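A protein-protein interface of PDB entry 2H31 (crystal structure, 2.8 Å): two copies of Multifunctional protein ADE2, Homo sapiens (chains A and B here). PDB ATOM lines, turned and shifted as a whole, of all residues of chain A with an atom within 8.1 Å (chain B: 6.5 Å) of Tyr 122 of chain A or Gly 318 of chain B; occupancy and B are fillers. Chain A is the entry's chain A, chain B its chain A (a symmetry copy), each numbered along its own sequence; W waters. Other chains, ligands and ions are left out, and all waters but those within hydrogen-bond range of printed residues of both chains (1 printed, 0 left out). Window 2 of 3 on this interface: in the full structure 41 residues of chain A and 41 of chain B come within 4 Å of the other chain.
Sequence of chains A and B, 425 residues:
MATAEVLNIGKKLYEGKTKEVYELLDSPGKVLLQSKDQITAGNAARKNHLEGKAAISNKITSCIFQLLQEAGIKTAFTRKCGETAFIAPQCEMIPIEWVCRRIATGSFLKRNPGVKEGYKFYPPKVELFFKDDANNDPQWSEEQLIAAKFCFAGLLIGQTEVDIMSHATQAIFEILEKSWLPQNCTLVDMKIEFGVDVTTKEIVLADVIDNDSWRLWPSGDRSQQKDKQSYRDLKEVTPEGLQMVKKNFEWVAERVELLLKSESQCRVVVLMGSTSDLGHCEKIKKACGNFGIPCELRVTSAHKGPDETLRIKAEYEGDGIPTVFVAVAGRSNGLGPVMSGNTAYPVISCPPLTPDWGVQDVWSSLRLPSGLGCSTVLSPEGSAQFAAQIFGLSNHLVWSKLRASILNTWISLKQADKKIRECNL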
ATOM      1  N   ARG A 101     -27.349 -11.347 -22.926  1.00  0.00           N
ATOM      2  CA  ARG A 101     -26.617 -12.171 -23.889  1.00  0.00           C
ATOM      3  C   ARG A 101     -25.125 -12.081 -23.754  1.00  0.00           C
ATOM      4  O   ARG A 101     -24.584 -11.032 -23.429  1.00  0.00           O
ATOM      5  CB  ARG A 101     -26.914 -11.743 -25.323  1.00  0.00           C
ATOM      6  CG  ARG A 101     -28.335 -11.842 -25.742  1.00  0.00           C
ATOM      7  CD  ARG A 101     -28.594 -11.041 -27.000  1.00  0.00           C
ATOM      8  NE  ARG A 101     -29.994 -11.191 -27.365  1.00  0.00           N
ATOM      9  CZ  ARG A 101     -30.545 -12.364 -27.657  1.00  0.00           C
ATOM     10  NH1 ARG A 101     -29.801 -13.469 -27.634  1.00  0.00           N
ATOM     11  NH2 ARG A 101     -31.841 -12.436 -27.942  1.00  0.00           N
ATOM     12  N   ARG A 102     -24.464 -13.191 -24.044  1.00  0.00           N
ATOM     13  CA  ARG A 102     -23.019 -13.236 -24.046  1.00  0.00           C
ATOM     14  C   ARG A 102     -22.673 -13.467 -25.514  1.00  0.00           C
ATOM     15  O   ARG A 102     -21.677 -12.956 -26.023  1.00  0.00           O
ATOM     16  CB  ARG A 102     -22.495 -14.395 -23.205  1.00  0.00           C
ATOM     17  CG  ARG A 102     -20.982 -14.576 -23.322  1.00  0.00           C
ATOM     18  CD  ARG A 102     -20.213 -13.390 -22.750  1.00  0.00           C
ATOM     19  NE  ARG A 102     -20.262 -13.352 -21.287  1.00  0.00           N
ATOM     20  CZ  ARG A 102     -19.747 -12.383 -20.535  1.00  0.00           C
ATOM     21  NH1 ARG A 102     -19.130 -11.345 -21.083  1.00  0.00           N
ATOM     22  NH2 ARG A 102     -19.853 -12.455 -19.222  1.00  0.00           N
ATOM     23  N   ILE A 103     -23.530 -14.236 -26.182  1.00  0.00           N
ATOM     24  CA  ILE A 103     -23.369 -14.585 -27.592  1.00  0.00           C
ATOM     25  C   ILE A 103     -24.660 -14.310 -28.352  1.00  0.00           C
ATOM     26  O   ILE A 103     -25.747 -14.617 -27.856  1.00  0.00           O
ATOM     27  CB  ILE A 103     -23.080 -16.079 -27.768  1.00  0.00           C
ATOM     28  CG1 ILE A 103     -21.856 -16.488 -26.959  1.00  0.00           C
ATOM     29  CG2 ILE A 103     -22.890 -16.387 -29.235  1.00  0.00           C
ATOM     30  CD1 ILE A 103     -21.641 -17.970 -26.958  1.00  0.00           C
ATOM     31  N   GLY A 118     -22.380 -15.720 -33.123  1.00  0.00           N
ATOM     32  CA  GLY A 118     -21.176 -15.962 -32.347  1.00  0.00           C
ATOM     33  C   GLY A 118     -20.570 -14.720 -31.705  1.00  0.00           C
ATOM     34  O   GLY A 118     -19.788 -14.818 -30.751  1.00  0.00           O
ATOM     35  N   TYR A 119     -20.922 -13.551 -32.230  1.00  0.00           N
ATOM     36  CA  TYR A 119     -20.414 -12.292 -31.710  1.00  0.00           C
ATOM     37  C   TYR A 119     -20.535 -12.288 -30.210  1.00  0.00           C
ATOM     38  O   TYR A 119     -21.626 -12.465 -29.667  1.00  0.00           O
ATOM     39  CB  TYR A 119     -21.224 -11.125 -32.251  1.00  0.00           C
ATOM     40  CG  TYR A 119     -20.687  -9.761 -31.890  1.00  0.00           C
ATOM     41  CD1 TYR A 119     -19.673  -9.174 -32.644  1.00  0.00           C
ATOM     42  CD2 TYR A 119     -21.241  -9.022 -30.843  1.00  0.00           C
ATOM     43  CE1 TYR A 119     -19.227  -7.875 -32.382  1.00  0.00           C
ATOM     44  CE2 TYR A 119     -20.805  -7.720 -30.566  1.00  0.00           C
ATOM     45  CZ  TYR A 119     -19.799  -7.150 -31.347  1.00  0.00           C
ATOM     46  OH  TYR A 119     -19.398  -5.846 -31.142  1.00  0.00           O
ATOM     47  N   LYS A 120     -19.418 -12.090 -29.530  1.00  0.00           N
ATOM     48  CA  LYS A 120     -19.461 -12.046 -28.087  1.00  0.00           C
ATOM     49  C   LYS A 120     -19.638 -10.623 -27.581  1.00  0.00           C
ATOM     50  O   LYS A 120     -19.008  -9.684 -28.069  1.00  0.00           O
ATOM     51  CB  LYS A 120     -18.200 -12.658 -27.505  1.00  0.00           C
ATOM     52  CG  LYS A 120     -18.171 -14.160 -27.607  1.00  0.00           C
ATOM     53  CD  LYS A 120     -17.196 -14.718 -26.596  1.00  0.00           C
ATOM     54  CE  LYS A 120     -17.286 -16.226 -26.509  1.00  0.00           C
ATOM     55  NZ  LYS A 120     -16.795 -16.876 -27.758  1.00  0.00           N
ATOM     56  N   PHE A 121     -20.545 -10.469 -26.624  1.00  0.00           N
ATOM     57  CA  PHE A 121     -20.803  -9.174 -26.008  1.00  0.00           C
ATOM     58  C   PHE A 121     -20.046  -9.204 -24.685  1.00  0.00           C
ATOM     59  O   PHE A 121     -20.212 -10.134 -23.888  1.00  0.00           O
ATOM     60  CB  PHE A 121     -22.297  -8.989 -25.763  1.00  0.00           C
ATOM     61  CG  PHE A 121     -23.099  -8.896 -27.010  1.00  0.00           C
ATOM     62  CD1 PHE A 121     -23.916  -9.947 -27.404  1.00  0.00           C
ATOM     63  CD2 PHE A 121     -23.053  -7.749 -27.790  1.00  0.00           C
ATOM     64  CE1 PHE A 121     -24.683  -9.858 -28.562  1.00  0.00           C
ATOM     65  CE2 PHE A 121     -23.813  -7.647 -28.946  1.00  0.00           C
ATOM     66  CZ  PHE A 121     -24.632  -8.705 -29.332  1.00  0.00           C
ATOM     67  N   TYR A 122     -19.216  -8.208 -24.420  1.00  0.00           N
ATOM     68  CA  TYR A 122     -18.478  -8.314 -23.187  1.00  0.00           C
ATOM     69  C   TYR A 122     -19.032  -7.718 -21.920  1.00  0.00           C
ATOM     70  O   TYR A 122     -18.830  -8.281 -20.836  1.00  0.00           O
ATOM     71  CB  TYR A 122     -17.023  -7.936 -23.421  1.00  0.00           C
ATOM     72  CG  TYR A 122     -16.340  -9.141 -24.014  1.00  0.00           C
ATOM     73  CD1 TYR A 122     -16.157  -9.261 -25.385  1.00  0.00           C
ATOM     74  CD2 TYR A 122     -16.025 -10.237 -23.212  1.00  0.00           C
ATOM     75  CE1 TYR A 122     -15.683 -10.444 -25.944  1.00  0.00           C
ATOM     76  CE2 TYR A 122     -15.557 -11.422 -23.757  1.00  0.00           C
ATOM     77  CZ  TYR A 122     -15.388 -11.520 -25.124  1.00  0.00           C
ATOM     78  OH  TYR A 122     -14.926 -12.695 -25.670  1.00  0.00           O
ATOM     79  N   PRO A 123     -19.738  -6.592 -22.012  1.00  0.00           N
ATOM     80  CA  PRO A 123     -20.213  -6.158 -20.701  1.00  0.00           C
ATOM     81  C   PRO A 123     -21.035  -7.163 -19.842  1.00  0.00           C
ATOM     82  O   PRO A 123     -20.847  -7.192 -18.624  1.00  0.00           O
ATOM     83  CB  PRO A 123     -20.926  -4.865 -21.029  1.00  0.00           C
ATOM     84  CG  PRO A 123     -19.938  -4.257 -22.004  1.00  0.00           C
ATOM     85  CD  PRO A 123     -19.577  -5.438 -22.914  1.00  0.00           C
ATOM     86  N   PRO A 124     -21.940  -7.998 -20.415  1.00  0.00           N
ATOM     87  CA  PRO A 124     -22.473  -8.309 -21.737  1.00  0.00           C
ATOM     88  C   PRO A 124     -23.861  -7.681 -21.910  1.00  0.00           C
ATOM     89  O   PRO A 124     -24.488  -7.257 -20.934  1.00  0.00           O
ATOM     90  CB  PRO A 124     -22.548  -9.822 -21.704  1.00  0.00           C
ATOM     91  CG  PRO A 124     -23.067 -10.059 -20.343  1.00  0.00           C
ATOM     92  CD  PRO A 124     -22.221  -9.131 -19.504  1.00  0.00           C
ATOM     93  N   LYS A 125     -24.338  -7.679 -23.155  1.00  0.00           N
ATOM     94  CA  LYS A 125     -25.616  -7.087 -23.557  1.00  0.00           C
ATOM     95  C   LYS A 125     -26.890  -7.393 -22.798  1.00  0.00           C
ATOM     96  O   LYS A 125     -27.240  -8.553 -22.571  1.00  0.00           O
ATOM     97  CB  LYS A 125     -25.866  -7.369 -25.035  1.00  0.00           C
ATOM     98  CG  LYS A 125     -25.215  -6.359 -25.969  1.00  0.00           C
ATOM     99  CD  LYS A 125     -25.788  -4.949 -25.816  1.00  0.00           C
ATOM    100  CE  LYS A 125     -27.256  -4.905 -26.211  1.00  0.00           C
ATOM    101  NZ  LYS A 125     -27.490  -5.446 -27.574  1.00  0.00           N
ATOM    102  N   GLN A 170     -27.631  -8.453 -15.375  1.00  0.00           N
ATOM    103  CA  GLN A 170     -26.279  -8.748 -15.812  1.00  0.00           C
ATOM    104  C   GLN A 170     -25.547  -9.562 -14.737  1.00  0.00           C
ATOM    105  O   GLN A 170     -24.834 -10.529 -15.034  1.00  0.00           O
ATOM    106  CB  GLN A 170     -25.570  -7.439 -16.062  1.00  0.00           C
ATOM    107  CG  GLN A 170     -24.357  -7.544 -16.902  1.00  0.00           C
ATOM    108  CD  GLN A 170     -23.749  -6.194 -17.078  1.00  0.00           C
ATOM    109  OE1 GLN A 170     -24.438  -5.240 -17.455  1.00  0.00           O
ATOM    110  NE2 GLN A 170     -22.457  -6.086 -16.793  1.00  0.00           N
ATOM    111  N   PHE A 173     -26.818 -13.022 -14.621  1.00  0.00           N
ATOM    112  CA  PHE A 173     -26.308 -13.726 -15.794  1.00  0.00           C
ATOM    113  C   PHE A 173     -24.938 -14.301 -15.490  1.00  0.00           C
ATOM    114  O   PHE A 173     -24.727 -15.514 -15.530  1.00  0.00           O
ATOM    115  CB  PHE A 173     -26.179 -12.772 -16.971  1.00  0.00           C
ATOM    116  CG  PHE A 173     -25.726 -13.438 -18.231  1.00  0.00           C
ATOM    117  CD1 PHE A 173     -26.643 -14.059 -19.067  1.00  0.00           C
ATOM    118  CD2 PHE A 173     -24.371 -13.480 -18.561  1.00  0.00           C
ATOM    119  CE1 PHE A 173     -26.220 -14.716 -20.211  1.00  0.00           C
ATOM    120  CE2 PHE A 173     -23.934 -14.134 -19.702  1.00  0.00           C
ATOM    121  CZ  PHE A 173     -24.860 -14.755 -20.531  1.00  0.00           C
ATOM    122  N   GLU A 174     -24.009 -13.403 -15.190  1.00  0.00           N
ATOM    123  CA  GLU A 174     -22.641 -13.777 -14.875  1.00  0.00           C
ATOM    124  C   GLU A 174     -22.550 -14.871 -13.806  1.00  0.00           C
ATOM    125  O   GLU A 174     -21.712 -15.769 -13.905  1.00  0.00           O
ATOM    126  CB  GLU A 174     -21.870 -12.531 -14.436  1.00  0.00           C
ATOM    127  CG  GLU A 174     -21.643 -11.549 -15.575  1.00  0.00           C
ATOM    128  CD  GLU A 174     -21.126 -10.197 -15.115  1.00  0.00           C
ATOM    129  OE1 GLU A 174     -20.223 -10.169 -14.237  1.00  0.00           O
ATOM    130  OE2 GLU A 174     -21.612  -9.166 -15.646  1.00  0.00           O
ATOM    131  N   GLU A 177     -23.683 -17.906 -15.469  1.00  0.00           N
ATOM    132  CA  GLU A 177     -22.701 -18.240 -16.483  1.00  0.00           C
ATOM    133  C   GLU A 177     -21.560 -18.992 -15.809  1.00  0.00           C
ATOM    134  O   GLU A 177     -21.144 -20.053 -16.277  1.00  0.00           O
ATOM    135  CB  GLU A 177     -22.149 -16.987 -17.154  1.00  0.00           C
ATOM    136  CG  GLU A 177     -21.232 -17.295 -18.321  1.00  0.00           C
ATOM    137  CD  GLU A 177     -20.759 -16.045 -19.036  1.00  0.00           C
ATOM    138  OE1 GLU A 177     -20.284 -16.164 -20.181  1.00  0.00           O
ATOM    139  OE2 GLU A 177     -20.852 -14.941 -18.456  1.00  0.00           O
ATOM    140  N   LYS A 178     -21.074 -18.442 -14.697  1.00  0.00           N
ATOM    141  CA  LYS A 178     -19.976 -19.043 -13.957  1.00  0.00           C
ATOM    142  C   LYS A 178     -20.365 -20.390 -13.386  1.00  0.00           C
ATOM    143  O   LYS A 178     -19.655 -21.374 -13.565  1.00  0.00           O
ATOM    144  CB  LYS A 178     -19.550 -18.128 -12.814  1.00  0.00           C
ATOM    145  CG  LYS A 178     -18.276 -18.564 -12.115  1.00  0.00           C
ATOM    146  CD  LYS A 178     -17.060 -18.343 -12.996  1.00  0.00           C
ATOM    147  CE  LYS A 178     -16.792 -16.864 -13.182  1.00  0.00           C
ATOM    148  NZ  LYS A 178     -15.574 -16.628 -13.999  1.00  0.00           N
ATOM    149  N   LEU A 181     -20.183 -23.267 -16.104  1.00  0.00           N
ATOM    150  CA  LEU A 181     -18.884 -23.679 -16.636  1.00  0.00           C
ATOM    151  C   LEU A 181     -18.328 -25.045 -16.226  1.00  0.00           C
ATOM    152  O   LEU A 181     -17.820 -25.779 -17.074  1.00  0.00           O
ATOM    153  CB  LEU A 181     -17.825 -22.604 -16.375  1.00  0.00           C
ATOM    154  CG  LEU A 181     -17.749 -21.544 -17.476  1.00  0.00           C
ATOM    155  CD1 LEU A 181     -16.327 -21.001 -17.494  1.00  0.00           C
ATOM    156  CD2 LEU A 181     -18.096 -22.137 -18.860  1.00  0.00           C
ATOM    157  N   TRP A 399     -17.076 -16.934  -6.014  1.00  0.00           N
ATOM    158  CA  TRP A 399     -17.127 -15.878  -7.008  1.00  0.00           C
ATOM    159  C   TRP A 399     -18.508 -15.237  -7.006  1.00  0.00           C
ATOM    160  O   TRP A 399     -18.639 -14.009  -7.061  1.00  0.00           O
ATOM    161  CB  TRP A 399     -16.849 -16.423  -8.414  1.00  0.00           C
ATOM    162  CG  TRP A 399     -17.410 -15.527  -9.521  1.00  0.00           C
ATOM    163  CD1 TRP A 399     -18.722 -15.456  -9.973  1.00  0.00           C
ATOM    164  CD2 TRP A 399     -16.695 -14.554 -10.254  1.00  0.00           C
ATOM    165  NE1 TRP A 399     -18.847 -14.491 -10.943  1.00  0.00           N
ATOM    166  CE2 TRP A 399     -17.619 -13.921 -11.136  1.00  0.00           C
ATOM    167  CE3 TRP A 399     -15.363 -14.145 -10.258  1.00  0.00           C
ATOM    168  CZ2 TRP A 399     -17.237 -12.900 -12.011  1.00  0.00           C
ATOM    169  CZ3 TRP A 399     -14.977 -13.116 -11.134  1.00  0.00           C
ATOM    170  CH2 TRP A 399     -15.908 -12.509 -11.996  1.00  0.00           C
ATOM    171  N   ARG B 311     -14.703  -1.097 -19.420  1.00  0.00           N
ATOM    172  CA  ARG B 311     -14.883  -1.886 -20.635  1.00  0.00           C
ATOM    173  C   ARG B 311     -13.822  -2.993 -20.776  1.00  0.00           C
ATOM    174  O   ARG B 311     -14.152  -4.168 -20.972  1.00  0.00           O
ATOM    175  CB  ARG B 311     -14.831  -0.998 -21.870  1.00  0.00           C
ATOM    176  CG  ARG B 311     -15.300  -1.723 -23.120  1.00  0.00           C
ATOM    177  CD  ARG B 311     -15.179  -0.862 -24.354  1.00  0.00           C
ATOM    178  NE  ARG B 311     -13.799  -0.730 -24.799  1.00  0.00           N
ATOM    179  CZ  ARG B 311     -13.035  -1.751 -25.176  1.00  0.00           C
ATOM    180  NH1 ARG B 311     -13.511  -2.987 -25.162  1.00  0.00           N
ATOM    181  NH2 ARG B 311     -11.792  -1.534 -25.586  1.00  0.00           N
ATOM    182  N   LYS B 313     -12.011  -4.174 -18.515  1.00  0.00           N
ATOM    183  CA  LYS B 313     -12.178  -5.100 -17.401  1.00  0.00           C
ATOM    184  C   LYS B 313     -13.147  -6.193 -17.848  1.00  0.00           C
ATOM    185  O   LYS B 313     -12.872  -7.386 -17.693  1.00  0.00           O
ATOM    186  CB  LYS B 313     -12.750  -4.365 -16.186  1.00  0.00           C
ATOM    187  CG  LYS B 313     -13.309  -5.279 -15.099  1.00  0.00           C
ATOM    188  CD  LYS B 313     -14.039  -4.475 -14.007  1.00  0.00           C
ATOM    189  CE  LYS B 313     -15.350  -3.828 -14.498  1.00  0.00           C
ATOM    190  NZ  LYS B 313     -16.485  -4.784 -14.675  1.00  0.00           N
ATOM    191  N   ALA B 314     -14.269  -5.766 -18.423  1.00  0.00           N
ATOM    192  CA  ALA B 314     -15.312  -6.681 -18.892  1.00  0.00           C
ATOM    193  C   ALA B 314     -14.852  -7.747 -19.899  1.00  0.00           C
ATOM    194  O   ALA B 314     -15.302  -8.901 -19.824  1.00  0.00           O
ATOM    195  CB  ALA B 314     -16.477  -5.884 -19.476  1.00  0.00           C
ATOM    196  N   GLU B 315     -13.967  -7.384 -20.832  1.00  0.00           N
ATOM    197  CA  GLU B 315     -13.517  -8.366 -21.807  1.00  0.00           C
ATOM    198  C   GLU B 315     -12.532  -9.396 -21.262  1.00  0.00           C
ATOM    199  O   GLU B 315     -12.218 -10.372 -21.933  1.00  0.00           O
ATOM    200  CB  GLU B 315     -12.972  -7.690 -23.073  1.00  0.00           C
ATOM    201  CG  GLU B 315     -11.910  -6.649 -22.886  1.00  0.00           C
ATOM    202  CD  GLU B 315     -11.649  -5.853 -24.173  1.00  0.00           C
ATOM    203  OE1 GLU B 315     -12.628  -5.338 -24.772  1.00  0.00           O
ATOM    204  OE2 GLU B 315     -10.465  -5.735 -24.579  1.00  0.00           O
ATOM    205  N   TYR B 316     -12.043  -9.186 -20.046  1.00  0.00           N
ATOM    206  CA  TYR B 316     -11.161 -10.159 -19.436  1.00  0.00           C
ATOM    207  C   TYR B 316     -12.032 -10.997 -18.517  1.00  0.00           C
ATOM    208  O   TYR B 316     -11.754 -12.164 -18.279  1.00  0.00           O
ATOM    209  CB  TYR B 316     -10.062  -9.477 -18.643  1.00  0.00           C
ATOM    210  CG  TYR B 316      -8.957  -8.954 -19.507  1.00  0.00           C
ATOM    211  CD1 TYR B 316      -8.110  -9.830 -20.193  1.00  0.00           C
ATOM    212  CD2 TYR B 316      -8.784  -7.576 -19.689  1.00  0.00           C
ATOM    213  CE1 TYR B 316      -7.121  -9.345 -21.050  1.00  0.00           C
ATOM    214  CE2 TYR B 316      -7.804  -7.079 -20.539  1.00  0.00           C
ATOM    215  CZ  TYR B 316      -6.983  -7.966 -21.218  1.00  0.00           C
ATOM    216  OH  TYR B 316      -6.064  -7.473 -22.094  1.00  0.00           O
ATOM    217  N   GLU B 317     -13.097 -10.394 -18.002  1.00  0.00           N
ATOM    218  CA  GLU B 317     -14.029 -11.103 -17.127  1.00  0.00           C
ATOM    219  C   GLU B 317     -14.902 -12.047 -17.949  1.00  0.00           C
ATOM    220  O   GLU B 317     -15.049 -13.228 -17.625  1.00  0.00           O
ATOM    221  CB  GLU B 317     -14.937 -10.116 -16.386  1.00  0.00           C
ATOM    222  CG  GLU B 317     -14.221  -9.251 -15.366  1.00  0.00           C
ATOM    223  CD  GLU B 317     -15.080  -8.101 -14.842  1.00  0.00           C
ATOM    224  OE1 GLU B 317     -14.754  -7.582 -13.751  1.00  0.00           O
ATOM    225  OE2 GLU B 317     -16.065  -7.711 -15.520  1.00  0.00           O
ATOM    226  N   GLY B 318     -15.469 -11.514 -19.026  1.00  0.00           N
ATOM    227  CA  GLY B 318     -16.347 -12.308 -19.864  1.00  0.00           C
ATOM    228  C   GLY B 318     -15.783 -13.501 -20.625  1.00  0.00           C
ATOM    229  O   GLY B 318     -16.559 -14.358 -21.044  1.00  0.00           O
ATOM    230  N   ASP B 319     -14.466 -13.579 -20.803  1.00  0.00           N
ATOM    231  CA  ASP B 319     -13.883 -14.682 -21.562  1.00  0.00           C
ATOM    232  C   ASP B 319     -13.506 -15.905 -20.735  1.00  0.00           C
ATOM    233  O   ASP B 319     -12.743 -16.763 -21.193  1.00  0.00           O
ATOM    234  CB  ASP B 319     -12.673 -14.191 -22.364  1.00  0.00           C
ATOM    235  CG  ASP B 319     -11.389 -14.143 -21.548  1.00  0.00           C
ATOM    236  OD1 ASP B 319     -11.449 -14.070 -20.303  1.00  0.00           O
ATOM    237  OD2 ASP B 319     -10.302 -14.160 -22.165  1.00  0.00           O
ATOM    238  N   GLY B 320     -14.031 -15.976 -19.515  1.00  0.00           N
ATOM    239  CA  GLY B 320     -13.773 -17.116 -18.649  1.00  0.00           C
ATOM    240  C   GLY B 320     -12.370 -17.527 -18.210  1.00  0.00           C
ATOM    241  O   GLY B 320     -12.248 -18.489 -17.460  1.00  0.00           O
ATOM    242  N   ILE B 321     -11.316 -16.852 -18.659  1.00  0.00           N
ATOM    243  CA  ILE B 321      -9.962 -17.217 -18.231  1.00  0.00           C
ATOM    244  C   ILE B 321      -9.694 -16.688 -16.819  1.00  0.00           C
ATOM    245  O   ILE B 321      -9.780 -15.486 -16.581  1.00  0.00           O
ATOM    246  CB  ILE B 321      -8.897 -16.611 -19.156  1.00  0.00           C
ATOM    247  CG1 ILE B 321      -9.040 -17.171 -20.557  1.00  0.00           C
ATOM    248  CG2 ILE B 321      -7.526 -16.930 -18.639  1.00  0.00           C
ATOM    249  CD1 ILE B 321      -8.762 -18.653 -20.614  1.00  0.00           C
ATOM    250  N   TYR B 345     -12.650 -10.626  -9.313  1.00  0.00           N
ATOM    251  CA  TYR B 345     -11.309 -11.225  -9.352  1.00  0.00           C
ATOM    252  C   TYR B 345     -10.322 -10.429  -8.456  1.00  0.00           C
ATOM    253  O   TYR B 345     -10.571  -9.271  -8.081  1.00  0.00           O
ATOM    254  CB  TYR B 345     -10.750 -11.251 -10.782  1.00  0.00           C
ATOM    255  CG  TYR B 345     -11.347 -12.287 -11.709  1.00  0.00           C
ATOM    256  CD1 TYR B 345     -11.735 -13.542 -11.238  1.00  0.00           C
ATOM    257  CD2 TYR B 345     -11.449 -12.041 -13.080  1.00  0.00           C
ATOM    258  CE1 TYR B 345     -12.208 -14.527 -12.118  1.00  0.00           C
ATOM    259  CE2 TYR B 345     -11.916 -13.014 -13.967  1.00  0.00           C
ATOM    260  CZ  TYR B 345     -12.292 -14.255 -13.480  1.00  0.00           C
ATOM    261  OH  TYR B 345     -12.732 -15.224 -14.352  1.00  0.00           O
HETATM  262  O   HOH W   1     -15.337 -13.538 -14.692  1.00  0.00           O
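The side-chain amino group (NZ) of Lys 178 of chain A sits at hydrogen-bond distance from the side-chain hydroxyl (OH) of Tyr 345 of chain B, at 3.2 Å.
Printed residues of chain A within 4 Å of Tyr 345 of chain B: Lys 178 (3.2 Å) and Trp 399 (3.3 Å). Printed residues of chain A within 4 Å of Glu 315 of chain B: Tyr 122 (3.4 Å). Of the printed residues of chain A, Ala 314 of chain B touches Tyr 122 (3.6 Å) and Pro 123 (3.9 Å). The nearest residue of chain A that does not touch Gly 318 of chain B is Glu 177 of chain A (4.2 Å).
Water W1 lies within hydrogen-bond range of O of Glu 317 of chain B, OH of Tyr 345 of chain B and NZ of Lys 178 of chain A.
The side-chain carboxylate (OE1) of Glu 315 of chain B is in salt-bridge range of the guanidinium group (NH1) of Arg 311 of chain B (2.5 Å). The guanidinium group (NH2) of Arg 102 of chain A lies within salt-bridge range of the side-chain carboxylate (OE2) of Glu 177 of chain A (2.8 Å). NE2 of Gln 170 of chain A sits at hydrogen-bond distance from O of Pro 123 of chain A (2.7 Å). NH1 of Arg 102 of chain A lies within hydrogen-bond range of O of Tyr 122 of chain A (3.1 Å). The side-chain carboxylate of Asp 319 of chain B sits close to the backbone NH of Ile 321 of chain B (3.2 Å). The backbone carbonyl oxygen (O) of Arg 102 of chain A is in hydrogen-bond range of the backbone NH (N) of Phe 121 of chain A (2.8 Å).
Hydrophobic or aromatic side chains of chain B within 4 Å of the printed part of chain A: Ala 314 and Tyr 345. Hydrophobic or aromatic side chains of chain A within 4 Å of the printed part of chain B: Tyr 122 and Trp 399. Among the printed residues, 8 pairs touch across the chains.
No position is printed for both chains. Of the 8 pairs that touch across the chains among the printed residues, none has its exchanged pair printed and touching as well.
Among the printed residues, merely in contact across the chains: Arg 102 of chain A with Gly 318 of chain B, Tyr 122 of chain A with Ala 314 of chain B, Tyr 122 of chain A with Glu 315 of chain B, Tyr 122 of chain A with Gly 318 of chain B, Tyr 122 of chain A with Asp 319 of chain B, Pro 123 of chain A with Ala 314 of chain B and Trp 399 of chain A with Tyr 345 of chain B.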
